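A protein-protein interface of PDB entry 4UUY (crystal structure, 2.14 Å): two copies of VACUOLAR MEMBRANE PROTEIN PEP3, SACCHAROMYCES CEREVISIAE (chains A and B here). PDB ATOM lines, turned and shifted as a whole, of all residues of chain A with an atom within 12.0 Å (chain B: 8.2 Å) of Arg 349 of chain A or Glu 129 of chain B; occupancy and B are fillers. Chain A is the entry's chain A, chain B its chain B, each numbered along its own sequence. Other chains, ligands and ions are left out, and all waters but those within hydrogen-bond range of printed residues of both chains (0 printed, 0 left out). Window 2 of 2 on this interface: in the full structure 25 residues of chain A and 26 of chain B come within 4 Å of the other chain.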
ATOM      1  N   GLU A 223       4.172 -20.505  21.591  1.00  0.00           N
ATOM      2  CA  GLU A 223       4.042 -21.638  22.561  1.00  0.00           C
ATOM      3  C   GLU A 223       2.608 -22.132  22.740  1.00  0.00           C
ATOM      4  O   GLU A 223       2.099 -22.865  21.883  1.00  0.00           O
ATOM      5  CB  GLU A 223       4.718 -21.382  23.921  1.00  0.00           C
ATOM      6  CG  GLU A 223       6.212 -21.656  23.910  1.00  0.00           C
ATOM      7  CD  GLU A 223       6.991 -20.757  24.854  1.00  0.00           C
ATOM      8  OE1 GLU A 223       6.404 -20.256  25.851  1.00  0.00           O
ATOM      9  OE2 GLU A 223       8.205 -20.553  24.601  1.00  0.00           O
ATOM     10  N   PHE A 269      -4.883 -19.090  10.746  1.00  0.00           N
ATOM     11  CA  PHE A 269      -5.362 -20.350  11.308  1.00  0.00           C
ATOM     12  C   PHE A 269      -5.378 -21.553  10.344  1.00  0.00           C
ATOM     13  O   PHE A 269      -5.802 -22.630  10.731  1.00  0.00           O
ATOM     14  CB  PHE A 269      -6.764 -20.135  11.925  1.00  0.00           C
ATOM     15  CG  PHE A 269      -6.787 -19.127  13.030  1.00  0.00           C
ATOM     16  CD1 PHE A 269      -6.232 -19.432  14.254  1.00  0.00           C
ATOM     17  CD2 PHE A 269      -7.341 -17.885  12.837  1.00  0.00           C
ATOM     18  CE1 PHE A 269      -6.220 -18.520  15.281  1.00  0.00           C
ATOM     19  CE2 PHE A 269      -7.329 -16.941  13.855  1.00  0.00           C
ATOM     20  CZ  PHE A 269      -6.763 -17.263  15.090  1.00  0.00           C
ATOM     21  N   LEU A 285      -5.920 -26.163  13.196  1.00  0.00           N
ATOM     22  CA  LEU A 285      -6.464 -26.573  14.465  1.00  0.00           C
ATOM     23  C   LEU A 285      -6.977 -28.020  14.453  1.00  0.00           C
ATOM     24  O   LEU A 285      -6.976 -28.685  15.488  1.00  0.00           O
ATOM     25  CB  LEU A 285      -7.563 -25.593  14.886  1.00  0.00           C
ATOM     26  CG  LEU A 285      -6.994 -24.182  15.146  1.00  0.00           C
ATOM     27  CD1 LEU A 285      -8.040 -23.117  14.950  1.00  0.00           C
ATOM     28  CD2 LEU A 285      -6.419 -24.103  16.551  1.00  0.00           C
ATOM     29  N   VAL A 343     -13.111 -20.702  13.376  1.00  0.00           N
ATOM     30  CA  VAL A 343     -12.364 -21.593  14.278  1.00  0.00           C
ATOM     31  C   VAL A 343     -12.520 -21.285  15.772  1.00  0.00           C
ATOM     32  O   VAL A 343     -11.862 -21.906  16.596  1.00  0.00           O
ATOM     33  CB  VAL A 343     -10.844 -21.578  13.965  1.00  0.00           C
ATOM     34  CG1 VAL A 343     -10.558 -22.090  12.546  1.00  0.00           C
ATOM     35  CG2 VAL A 343     -10.236 -20.193  14.180  1.00  0.00           C
ATOM     36  N   TRP A 344     -13.357 -20.318  16.128  1.00  0.00           N
ATOM     37  CA  TRP A 344     -13.409 -19.877  17.524  1.00  0.00           C
ATOM     38  C   TRP A 344     -13.719 -21.021  18.507  1.00  0.00           C
ATOM     39  O   TRP A 344     -13.077 -21.148  19.566  1.00  0.00           O
ATOM     40  CB  TRP A 344     -14.404 -18.749  17.703  1.00  0.00           C
ATOM     41  CG  TRP A 344     -14.251 -18.051  19.037  1.00  0.00           C
ATOM     42  CD1 TRP A 344     -13.415 -17.021  19.324  1.00  0.00           C
ATOM     43  CD2 TRP A 344     -14.937 -18.357  20.260  1.00  0.00           C
ATOM     44  NE1 TRP A 344     -13.539 -16.651  20.632  1.00  0.00           N
ATOM     45  CE2 TRP A 344     -14.468 -17.453  21.236  1.00  0.00           C
ATOM     46  CE3 TRP A 344     -15.906 -19.303  20.625  1.00  0.00           C
ATOM     47  CZ2 TRP A 344     -14.929 -17.465  22.556  1.00  0.00           C
ATOM     48  CZ3 TRP A 344     -16.377 -19.309  21.938  1.00  0.00           C
ATOM     49  CH2 TRP A 344     -15.886 -18.395  22.888  1.00  0.00           C
ATOM     50  N   ASN A 345     -14.671 -21.870  18.143  1.00  0.00           N
ATOM     51  CA  ASN A 345     -15.032 -22.993  18.993  1.00  0.00           C
ATOM     52  C   ASN A 345     -13.850 -23.901  19.283  1.00  0.00           C
ATOM     53  O   ASN A 345     -13.801 -24.523  20.335  1.00  0.00           O
ATOM     54  CB  ASN A 345     -16.187 -23.778  18.393  1.00  0.00           C
ATOM     55  CG  ASN A 345     -17.499 -23.005  18.418  1.00  0.00           C
ATOM     56  OD1 ASN A 345     -17.676 -22.039  19.176  1.00  0.00           O
ATOM     57  ND2 ASN A 345     -18.451 -23.450  17.599  1.00  0.00           N
ATOM     58  N   LEU A 346     -12.875 -23.944  18.375  1.00  0.00           N
ATOM     59  CA  LEU A 346     -11.671 -24.757  18.577  1.00  0.00           C
ATOM     60  C   LEU A 346     -10.519 -24.067  19.322  1.00  0.00           C
ATOM     61  O   LEU A 346      -9.557 -24.721  19.709  1.00  0.00           O
ATOM     62  CB  LEU A 346     -11.174 -25.269  17.227  1.00  0.00           C
ATOM     63  CG  LEU A 346     -12.102 -26.241  16.482  1.00  0.00           C
ATOM     64  CD1 LEU A 346     -11.557 -26.477  15.084  1.00  0.00           C
ATOM     65  CD2 LEU A 346     -12.248 -27.562  17.231  1.00  0.00           C
ATOM     66  N   LEU A 347     -10.595 -22.756  19.507  1.00  0.00           N
ATOM     67  CA  LEU A 347      -9.579 -22.048  20.261  1.00  0.00           C
ATOM     68  C   LEU A 347      -9.753 -22.222  21.765  1.00  0.00           C
ATOM     69  O   LEU A 347      -8.775 -22.154  22.507  1.00  0.00           O
ATOM     70  CB  LEU A 347      -9.582 -20.562  19.898  1.00  0.00           C
ATOM     71  CG  LEU A 347      -9.300 -20.240  18.429  1.00  0.00           C
ATOM     72  CD1 LEU A 347      -9.442 -18.752  18.136  1.00  0.00           C
ATOM     73  CD2 LEU A 347      -7.927 -20.744  18.020  1.00  0.00           C
ATOM     74  N   VAL A 348     -10.979 -22.459  22.222  1.00  0.00           N
ATOM     75  CA  VAL A 348     -11.228 -22.579  23.668  1.00  0.00           C
ATOM     76  C   VAL A 348     -10.471 -23.800  24.234  1.00  0.00           C
ATOM     77  O   VAL A 348     -10.513 -24.886  23.653  1.00  0.00           O
ATOM     78  CB  VAL A 348     -12.731 -22.594  24.003  1.00  0.00           C
ATOM     79  CG1 VAL A 348     -13.424 -21.354  23.435  1.00  0.00           C
ATOM     80  CG2 VAL A 348     -13.410 -23.861  23.498  1.00  0.00           C
ATOM     81  N   ARG A 349      -9.767 -23.617  25.356  1.00  0.00           N
ATOM     82  CA  ARG A 349      -8.649 -24.526  25.727  1.00  0.00           C
ATOM     83  C   ARG A 349      -9.002 -26.013  25.850  1.00  0.00           C
ATOM     84  O   ARG A 349     -10.034 -26.381  26.409  1.00  0.00           O
ATOM     85  CB  ARG A 349      -7.928 -24.041  27.003  1.00  0.00           C
ATOM     86  CG  ARG A 349      -8.751 -24.086  28.284  1.00  0.00           C
ATOM     87  CD  ARG A 349      -7.954 -23.554  29.477  1.00  0.00           C
ATOM     88  NE  ARG A 349      -7.043 -24.546  30.050  1.00  0.00           N
ATOM     89  CZ  ARG A 349      -7.395 -25.516  30.900  1.00  0.00           C
ATOM     90  NH1 ARG A 349      -8.657 -25.668  31.296  1.00  0.00           N
ATOM     91  NH2 ARG A 349      -6.476 -26.355  31.360  1.00  0.00           N
ATOM     92  N   LEU B  87     -21.944 -11.832  24.913  1.00  0.00           N
ATOM     93  CA  LEU B  87     -21.151 -12.071  23.711  1.00  0.00           C
ATOM     94  C   LEU B  87     -22.046 -12.068  22.493  1.00  0.00           C
ATOM     95  O   LEU B  87     -23.117 -12.650  22.508  1.00  0.00           O
ATOM     96  CB  LEU B  87     -20.458 -13.416  23.767  1.00  0.00           C
ATOM     97  CG  LEU B  87     -19.407 -13.578  24.837  1.00  0.00           C
ATOM     98  CD1 LEU B  87     -18.820 -14.981  24.747  1.00  0.00           C
ATOM     99  CD2 LEU B  87     -18.335 -12.515  24.678  1.00  0.00           C
ATOM    100  N   LEU B  96     -23.579 -13.241  29.902  1.00  0.00           N
ATOM    101  CA  LEU B  96     -22.571 -13.676  30.861  1.00  0.00           C
ATOM    102  C   LEU B  96     -22.995 -13.192  32.251  1.00  0.00           C
ATOM    103  O   LEU B  96     -22.540 -12.158  32.748  1.00  0.00           O
ATOM    104  CB  LEU B  96     -21.195 -13.136  30.465  1.00  0.00           C
ATOM    105  CG  LEU B  96     -20.682 -13.506  29.063  1.00  0.00           C
ATOM    106  CD1 LEU B  96     -19.453 -12.697  28.721  1.00  0.00           C
ATOM    107  CD2 LEU B  96     -20.365 -14.984  28.950  1.00  0.00           C
ATOM    108  N   LYS B  98     -22.372 -14.293  35.128  1.00  0.00           N
ATOM    109  CA  LYS B  98     -21.358 -14.358  36.167  1.00  0.00           C
ATOM    110  C   LYS B  98     -20.681 -13.004  36.428  1.00  0.00           C
ATOM    111  O   LYS B  98     -20.076 -12.800  37.490  1.00  0.00           O
ATOM    112  CB  LYS B  98     -20.307 -15.407  35.807  1.00  0.00           C
ATOM    113  CG  LYS B  98     -19.456 -15.884  36.977  1.00  0.00           C
ATOM    114  CD  LYS B  98     -18.419 -16.902  36.528  1.00  0.00           C
ATOM    115  CE  LYS B  98     -19.043 -18.247  36.197  1.00  0.00           C
ATOM    116  NZ  LYS B  98     -18.074 -19.097  35.448  1.00  0.00           N
ATOM    117  N   TRP B 109      -7.537  -7.436  25.447  1.00  0.00           N
ATOM    118  CA  TRP B 109      -7.498  -8.800  24.889  1.00  0.00           C
ATOM    119  C   TRP B 109      -6.087  -9.301  24.753  1.00  0.00           C
ATOM    120  O   TRP B 109      -5.229  -8.574  24.298  1.00  0.00           O
ATOM    121  CB  TRP B 109      -8.137  -8.853  23.491  1.00  0.00           C
ATOM    122  CG  TRP B 109      -9.557  -8.556  23.482  1.00  0.00           C
ATOM    123  CD1 TRP B 109     -10.137  -7.328  23.305  1.00  0.00           C
ATOM    124  CD2 TRP B 109     -10.621  -9.489  23.658  1.00  0.00           C
ATOM    125  NE1 TRP B 109     -11.506  -7.445  23.367  1.00  0.00           N
ATOM    126  CE2 TRP B 109     -11.831  -8.759  23.575  1.00  0.00           C
ATOM    127  CE3 TRP B 109     -10.674 -10.884  23.847  1.00  0.00           C
ATOM    128  CZ2 TRP B 109     -13.079  -9.367  23.688  1.00  0.00           C
ATOM    129  CZ3 TRP B 109     -11.913 -11.488  23.978  1.00  0.00           C
ATOM    130  CH2 TRP B 109     -13.111 -10.727  23.900  1.00  0.00           C
ATOM    131  N   ASN B 111      -5.867 -12.674  23.357  1.00  0.00           N
ATOM    132  CA  ASN B 111      -6.116 -13.445  22.138  1.00  0.00           C
ATOM    133  C   ASN B 111      -7.638 -13.533  21.900  1.00  0.00           C
ATOM    134  O   ASN B 111      -8.389 -12.743  22.461  1.00  0.00           O
ATOM    135  CB  ASN B 111      -5.450 -14.824  22.224  1.00  0.00           C
ATOM    136  CG  ASN B 111      -5.922 -15.633  23.407  1.00  0.00           C
ATOM    137  OD1 ASN B 111      -7.114 -15.762  23.654  1.00  0.00           O
ATOM    138  ND2 ASN B 111      -4.987 -16.208  24.131  1.00  0.00           N
ATOM    139  N   GLU B 112      -8.094 -14.460  21.069  1.00  0.00           N
ATOM    140  CA  GLU B 112      -9.504 -14.493  20.726  1.00  0.00           C
ATOM    141  C   GLU B 112     -10.418 -15.023  21.834  1.00  0.00           C
ATOM    142  O   GLU B 112     -11.627 -14.950  21.694  1.00  0.00           O
ATOM    143  CB  GLU B 112      -9.728 -15.307  19.447  1.00  0.00           C
ATOM    144  CG  GLU B 112      -9.044 -14.701  18.233  1.00  0.00           C
ATOM    145  CD  GLU B 112      -9.468 -13.281  17.978  1.00  0.00           C
ATOM    146  OE1 GLU B 112     -10.626 -13.070  17.554  1.00  0.00           O
ATOM    147  OE2 GLU B 112      -8.640 -12.373  18.180  1.00  0.00           O
ATOM    148  N   THR B 113      -9.848 -15.571  22.905  1.00  0.00           N
ATOM    149  CA  THR B 113     -10.637 -16.151  23.973  1.00  0.00           C
ATOM    150  C   THR B 113     -10.292 -15.622  25.353  1.00  0.00           C
ATOM    151  O   THR B 113     -10.904 -16.048  26.339  1.00  0.00           O
ATOM    152  CB  THR B 113     -10.438 -17.676  24.052  1.00  0.00           C
ATOM    153  OG1 THR B 113      -9.080 -17.935  24.429  1.00  0.00           O
ATOM    154  CG2 THR B 113     -10.776 -18.354  22.714  1.00  0.00           C
ATOM    155  N   THR B 114      -9.362 -14.676  25.435  1.00  0.00           N
ATOM    156  CA  THR B 114      -8.773 -14.338  26.713  1.00  0.00           C
ATOM    157  C   THR B 114      -8.514 -12.843  26.831  1.00  0.00           C
ATOM    158  O   THR B 114      -7.964 -12.246  25.927  1.00  0.00           O
ATOM    159  CB  THR B 114      -7.461 -15.112  26.884  1.00  0.00           C
ATOM    160  OG1 THR B 114      -7.733 -16.518  26.760  1.00  0.00           O
ATOM    161  CG2 THR B 114      -6.816 -14.835  28.243  1.00  0.00           C
ATOM    162  N   PHE B 115      -8.909 -12.240  27.942  1.00  0.00           N
ATOM    163  CA  PHE B 115      -8.572 -10.834  28.185  1.00  0.00           C
ATOM    164  C   PHE B 115      -8.211 -10.584  29.634  1.00  0.00           C
ATOM    165  O   PHE B 115      -8.535 -11.374  30.516  1.00  0.00           O
ATOM    166  CB  PHE B 115      -9.700  -9.903  27.719  1.00  0.00           C
ATOM    167  CG  PHE B 115     -11.026 -10.140  28.394  1.00  0.00           C
ATOM    168  CD1 PHE B 115     -11.318  -9.547  29.621  1.00  0.00           C
ATOM    169  CD2 PHE B 115     -12.007 -10.913  27.777  1.00  0.00           C
ATOM    170  CE1 PHE B 115     -12.549  -9.733  30.230  1.00  0.00           C
ATOM    171  CE2 PHE B 115     -13.242 -11.108  28.382  1.00  0.00           C
ATOM    172  CZ  PHE B 115     -13.512 -10.509  29.612  1.00  0.00           C
ATOM    173  N   LEU B 116      -7.515  -9.476  29.852  1.00  0.00           N
ATOM    174  CA  LEU B 116      -7.169  -9.011  31.181  1.00  0.00           C
ATOM    175  C   LEU B 116      -8.084  -7.846  31.507  1.00  0.00           C
ATOM    176  O   LEU B 116      -8.398  -7.034  30.634  1.00  0.00           O
ATOM    177  CB  LEU B 116      -5.710  -8.572  31.230  1.00  0.00           C
ATOM    178  CG  LEU B 116      -4.671  -9.641  30.907  1.00  0.00           C
ATOM    179  CD1 LEU B 116      -3.304  -9.001  30.803  1.00  0.00           C
ATOM    180  CD2 LEU B 116      -4.665 -10.738  31.972  1.00  0.00           C
ATOM    181  N   TYR B 126      -7.506  -9.100  36.743  1.00  0.00           N
ATOM    182  CA  TYR B 126      -7.956 -10.491  36.568  1.00  0.00           C
ATOM    183  C   TYR B 126      -7.817 -10.962  35.140  1.00  0.00           C
ATOM    184  O   TYR B 126      -8.090 -10.220  34.201  1.00  0.00           O
ATOM    185  CB  TYR B 126      -9.437 -10.638  36.933  1.00  0.00           C
ATOM    186  CG  TYR B 126      -9.756 -10.439  38.388  1.00  0.00           C
ATOM    187  CD1 TYR B 126      -9.701 -11.501  39.274  1.00  0.00           C
ATOM    188  CD2 TYR B 126     -10.107  -9.198  38.877  1.00  0.00           C
ATOM    189  CE1 TYR B 126     -10.001 -11.340  40.605  1.00  0.00           C
ATOM    190  CE2 TYR B 126     -10.408  -9.014  40.223  1.00  0.00           C
ATOM    191  CZ  TYR B 126     -10.343 -10.085  41.078  1.00  0.00           C
ATOM    192  OH  TYR B 126     -10.649  -9.928  42.398  1.00  0.00           O
ATOM    193  N   ARG B 127      -7.431 -12.211  34.969  1.00  0.00           N
ATOM    194  CA  ARG B 127      -7.444 -12.801  33.640  1.00  0.00           C
ATOM    195  C   ARG B 127      -8.786 -13.507  33.471  1.00  0.00           C
ATOM    196  O   ARG B 127      -9.205 -14.256  34.339  1.00  0.00           O
ATOM    197  CB  ARG B 127      -6.268 -13.765  33.472  1.00  0.00           C
ATOM    198  CG  ARG B 127      -6.226 -14.482  32.129  1.00  0.00           C
ATOM    199  CD  ARG B 127      -5.263 -15.668  32.161  1.00  0.00           C
ATOM    200  NE  ARG B 127      -5.710 -16.782  31.306  1.00  0.00           N
ATOM    201  CZ  ARG B 127      -5.108 -17.200  30.192  1.00  0.00           C
ATOM    202  NH1 ARG B 127      -3.999 -16.617  29.739  1.00  0.00           N
ATOM    203  NH2 ARG B 127      -5.615 -18.222  29.518  1.00  0.00           N
ATOM    204  N   VAL B 128      -9.451 -13.231  32.352  1.00  0.00           N
ATOM    205  CA  VAL B 128     -10.705 -13.869  31.990  1.00  0.00           C
ATOM    206  C   VAL B 128     -10.560 -14.688  30.696  1.00  0.00           C
ATOM    207  O   VAL B 128     -10.046 -14.210  29.685  1.00  0.00           O
ATOM    208  CB  VAL B 128     -11.821 -12.829  31.793  1.00  0.00           C
ATOM    209  CG1 VAL B 128     -13.175 -13.517  31.619  1.00  0.00           C
ATOM    210  CG2 VAL B 128     -11.881 -11.871  32.980  1.00  0.00           C
ATOM    211  N   GLU B 129     -11.057 -15.911  30.741  1.00  0.00           N
ATOM    212  CA  GLU B 129     -11.022 -16.828  29.612  1.00  0.00           C
ATOM    213  C   GLU B 129     -12.463 -17.192  29.252  1.00  0.00           C
ATOM    214  O   GLU B 129     -13.247 -17.550  30.130  1.00  0.00           O
ATOM    215  CB  GLU B 129     -10.289 -18.075  30.065  1.00  0.00           C
ATOM    216  CG  GLU B 129      -9.571 -18.865  29.008  1.00  0.00           C
ATOM    217  CD  GLU B 129      -8.903 -20.066  29.639  1.00  0.00           C
ATOM    218  OE1 GLU B 129      -7.784 -19.917  30.173  1.00  0.00           O
ATOM    219  OE2 GLU B 129      -9.522 -21.138  29.658  1.00  0.00           O
ATOM    220  N   LEU B 130     -12.824 -17.038  27.985  1.00  0.00           N
ATOM    221  CA  LEU B 130     -14.159 -17.351  27.533  1.00  0.00           C
ATOM    222  C   LEU B 130     -14.192 -18.831  27.178  1.00  0.00           C
ATOM    223  O   LEU B 130     -13.269 -19.337  26.514  1.00  0.00           O
ATOM    224  CB  LEU B 130     -14.532 -16.515  26.317  1.00  0.00           C
ATOM    225  CG  LEU B 130     -14.469 -14.993  26.470  1.00  0.00           C
ATOM    226  CD1 LEU B 130     -14.662 -14.314  25.113  1.00  0.00           C
ATOM    227  CD2 LEU B 130     -15.501 -14.481  27.453  1.00  0.00           C
ATOM    228  N   THR B 131     -15.246 -19.520  27.630  1.00  0.00           N
ATOM    229  CA  THR B 131     -15.454 -20.940  27.342  1.00  0.00           C
ATOM    230  C   THR B 131     -16.535 -21.177  26.281  1.00  0.00           C
ATOM    231  O   THR B 131     -16.712 -22.309  25.845  1.00  0.00           O
ATOM    232  CB  THR B 131     -15.895 -21.698  28.596  1.00  0.00           C
ATOM    233  OG1 THR B 131     -17.104 -21.108  29.087  1.00  0.00           O
ATOM    234  CG2 THR B 131     -14.820 -21.650  29.678  1.00  0.00           C
ATOM    235  N   GLY B 132     -17.237 -20.122  25.866  1.00  0.00           N
ATOM    236  CA  GLY B 132     -18.349 -20.231  24.914  1.00  0.00           C
ATOM    237  C   GLY B 132     -19.659 -19.861  25.591  1.00  0.00           C
ATOM    238  O   GLY B 132     -20.298 -18.857  25.238  1.00  0.00           O
ATOM    239  N   LYS B 133     -20.031 -20.668  26.585  1.00  0.00           N
ATOM    240  CA  LYS B 133     -21.209 -20.423  27.422  1.00  0.00           C
ATOM    241  C   LYS B 133     -20.903 -19.525  28.620  1.00  0.00           C
ATOM    242  O   LYS B 133     -21.820 -18.931  29.201  1.00  0.00           O
ATOM    243  CB  LYS B 133     -21.762 -21.746  27.980  1.00  0.00           C
ATOM    244  CG  LYS B 133     -22.254 -22.760  26.951  1.00  0.00           C
ATOM    245  CD  LYS B 133     -23.568 -22.353  26.288  1.00  0.00           C
ATOM    246  CE  LYS B 133     -24.783 -22.604  27.167  1.00  0.00           C
ATOM    247  NZ  LYS B 133     -25.188 -24.035  27.203  1.00  0.00           N
ATOM    248  N   ASP B 134     -19.635 -19.450  29.018  1.00  0.00           N
ATOM    249  CA  ASP B 134     -19.294 -18.888  30.325  1.00  0.00           C
ATOM    250  C   ASP B 134     -17.850 -18.432  30.344  1.00  0.00           C
ATOM    251  O   ASP B 134     -17.221 -18.341  29.299  1.00  0.00           O
ATOM    252  CB  ASP B 134     -19.521 -19.948  31.417  1.00  0.00           C
ATOM    253  CG  ASP B 134     -19.926 -19.345  32.771  1.00  0.00           C
ATOM    254  OD1 ASP B 134     -19.635 -18.154  33.055  1.00  0.00           O
ATOM    255  OD2 ASP B 134     -20.526 -20.097  33.573  1.00  0.00           O
ATOM    256  N   ILE B 135     -17.328 -18.159  31.538  1.00  0.00           N
ATOM    257  CA  ILE B 135     -15.985 -17.645  31.698  1.00  0.00           C
ATOM    258  C   ILE B 135     -15.327 -18.355  32.860  1.00  0.00           C
ATOM    259  O   ILE B 135     -16.017 -18.937  33.674  1.00  0.00           O
ATOM    260  CB  ILE B 135     -16.011 -16.128  31.972  1.00  0.00           C
ATOM    261  CG1 ILE B 135     -16.697 -15.828  33.314  1.00  0.00           C
ATOM    262  CG2 ILE B 135     -16.731 -15.400  30.846  1.00  0.00           C
ATOM    263  CD1 ILE B 135     -16.411 -14.430  33.819  1.00  0.00           C
ATOM    264  N   THR B 136     -13.999 -18.323  32.906  1.00  0.00           N
ATOM    265  CA  THR B 136     -13.224 -18.681  34.099  1.00  0.00           C
ATOM    266  C   THR B 136     -12.403 -17.443  34.429  1.00  0.00           C
ATOM    267  O   THR B 136     -12.191 -16.607  33.558  1.00  0.00           O
ATOM    268  CB  THR B 136     -12.226 -19.817  33.834  1.00  0.00           C
ATOM    269  OG1 THR B 136     -11.339 -19.409  32.791  1.00  0.00           O
ATOM    270  CG2 THR B 136     -12.946 -21.101  33.422  1.00  0.00           C
ATOM    271  N   THR B 137     -11.948 -17.332  35.673  1.00  0.00           N
ATOM    272  CA  THR B 137     -11.193 -16.162  36.125  1.00  0.00           C
ATOM    273  C   THR B 137     -10.005 -16.562  36.958  1.00  0.00           C
ATOM    274  O   THR B 137     -10.005 -17.629  37.557  1.00  0.00           O
ATOM    275  CB  THR B 137     -12.035 -15.221  36.997  1.00  0.00           C
ATOM    276  OG1 THR B 137     -12.406 -15.898  38.202  1.00  0.00           O
ATOM    277  CG2 THR B 137     -13.276 -14.727  36.247  1.00  0.00           C
ATOM    278  N   LYS B 138      -9.008 -15.680  36.987  1.00  0.00           N
ATOM    279  CA  LYS B 138      -7.837 -15.826  37.826  1.00  0.00           C
ATOM    280  C   LYS B 138      -7.271 -14.444  38.173  1.00  0.00           C
ATOM    281  O   LYS B 138      -7.107 -13.599  37.281  1.00  0.00           O
ATOM    282  CB  LYS B 138      -6.761 -16.611  37.103  1.00  0.00           C
ATOM    283  CG  LYS B 138      -5.605 -16.983  38.018  1.00  0.00           C
ATOM    284  CD  LYS B 138      -4.361 -17.413  37.256  1.00  0.00           C
ATOM    285  CE  LYS B 138      -3.227 -17.682  38.242  1.00  0.00           C
ATOM    286  NZ  LYS B 138      -2.030 -18.294  37.595  1.00  0.00           N
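The side-chain amide oxygen (OD1) of Asn 111 of chain B is in hydrogen-bond range of the backbone NH (N) of Thr 113 of chain B (2.8 Å). The side-chain hydroxyl (OG1) of Thr 114 of chain B sits at hydrogen-bond distance from the side-chain hydroxyl (OG1) of Thr 113 of chain B, at 3.0 Å. O of Thr 113 of chain B lies within hydrogen-bond range of N of Leu 130 of chain B (2.7 Å). The guanidinium group of Arg 127 of chain B lies within salt-bridge range of the side-chain carboxylate of Glu 129 of chain B (2.8 Å). The backbone carbonyl oxygen (O) of Glu 129 of chain B sits at hydrogen-bond distance from the backbone NH (N) of Thr 136 of chain B, at 3.0 Å.
Hydrophobic or aromatic side chains of chain A that line the printed part of chain B: Trp 344, Leu 347 and Val 348. Along chain A the printed residues that touch a printed residue of chain B span positions 344 to 349. Printed residues of chain B that touch a printed residue of chain A: Glu 112, Thr 113, Glu 129, Leu 130 and Gly 132. Hydrophobic or aromatic side chains of chain B within 4 Å of the printed part of chain A: Leu 130. Among the printed residues, no Asp or Glu carboxylate lies within 4 Å of a Lys or Arg side-chain nitrogen of the other chain.
The indole nitrogen (NE1) of Trp 344 of chain A lies within hydrogen-bond range of the backbone carbonyl oxygen (O) of Glu 112 of chain B (2.8 Å).
Printed residues of chain B within 4 Å of Trp 344 of chain A: Glu 112, Thr 113, Leu 130 and Gly 132. Printed residues of chain B within 4 Å of Leu 347 of chain A: Glu 112 and Thr 113. Of the printed residues of chain B, Arg 349 of chain A touches Glu 129. Printed residues of chain A within 4 Å of Glu 112 of chain B: Trp 344 and Leu 347. Of chain A, only Trp 344 (3.9 Å) and Leu 347 (3.8 Å) come within 4 Å of Thr 113 of chain B. No residue of chain A comes within 4 Å of Thr 114 of chain B. Glu 129 of chain B touches just one residue of chain A: Arg 349 (2.9 Å). Leu 130 of chain B touches two residues of chain A. No residue of chain A comes within 4 Å of Ile 135 of chain B. No residue of chain A comes within 4 Å of Thr 136 of chain B. No residue of chain A comes within 4 Å of Thr 137 of chain B. The nearest printed residue of chain A that does not touch Glu 112 of chain B is Phe 269 of chain A (4.7 Å).
No position is printed for both chains. Of the 8 pairs that touch across the chains among the printed residues, none has its exchanged pair printed and touching as well.
Among the printed residues, merely in contact across the chains: Trp 344 of chain A with Thr 113 of chain B, Trp 344 of chain A with Leu 130 of chain B, Trp 344 of chain A with Gly 132 of chain B, Leu 347 of chain A with Glu 112 of chain B, Leu 347 of chain A with Thr 113 of chain B, Val 348 of chain A with Leu 130 of chain B and Arg 349 of chain A with Glu 129 of chain B.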
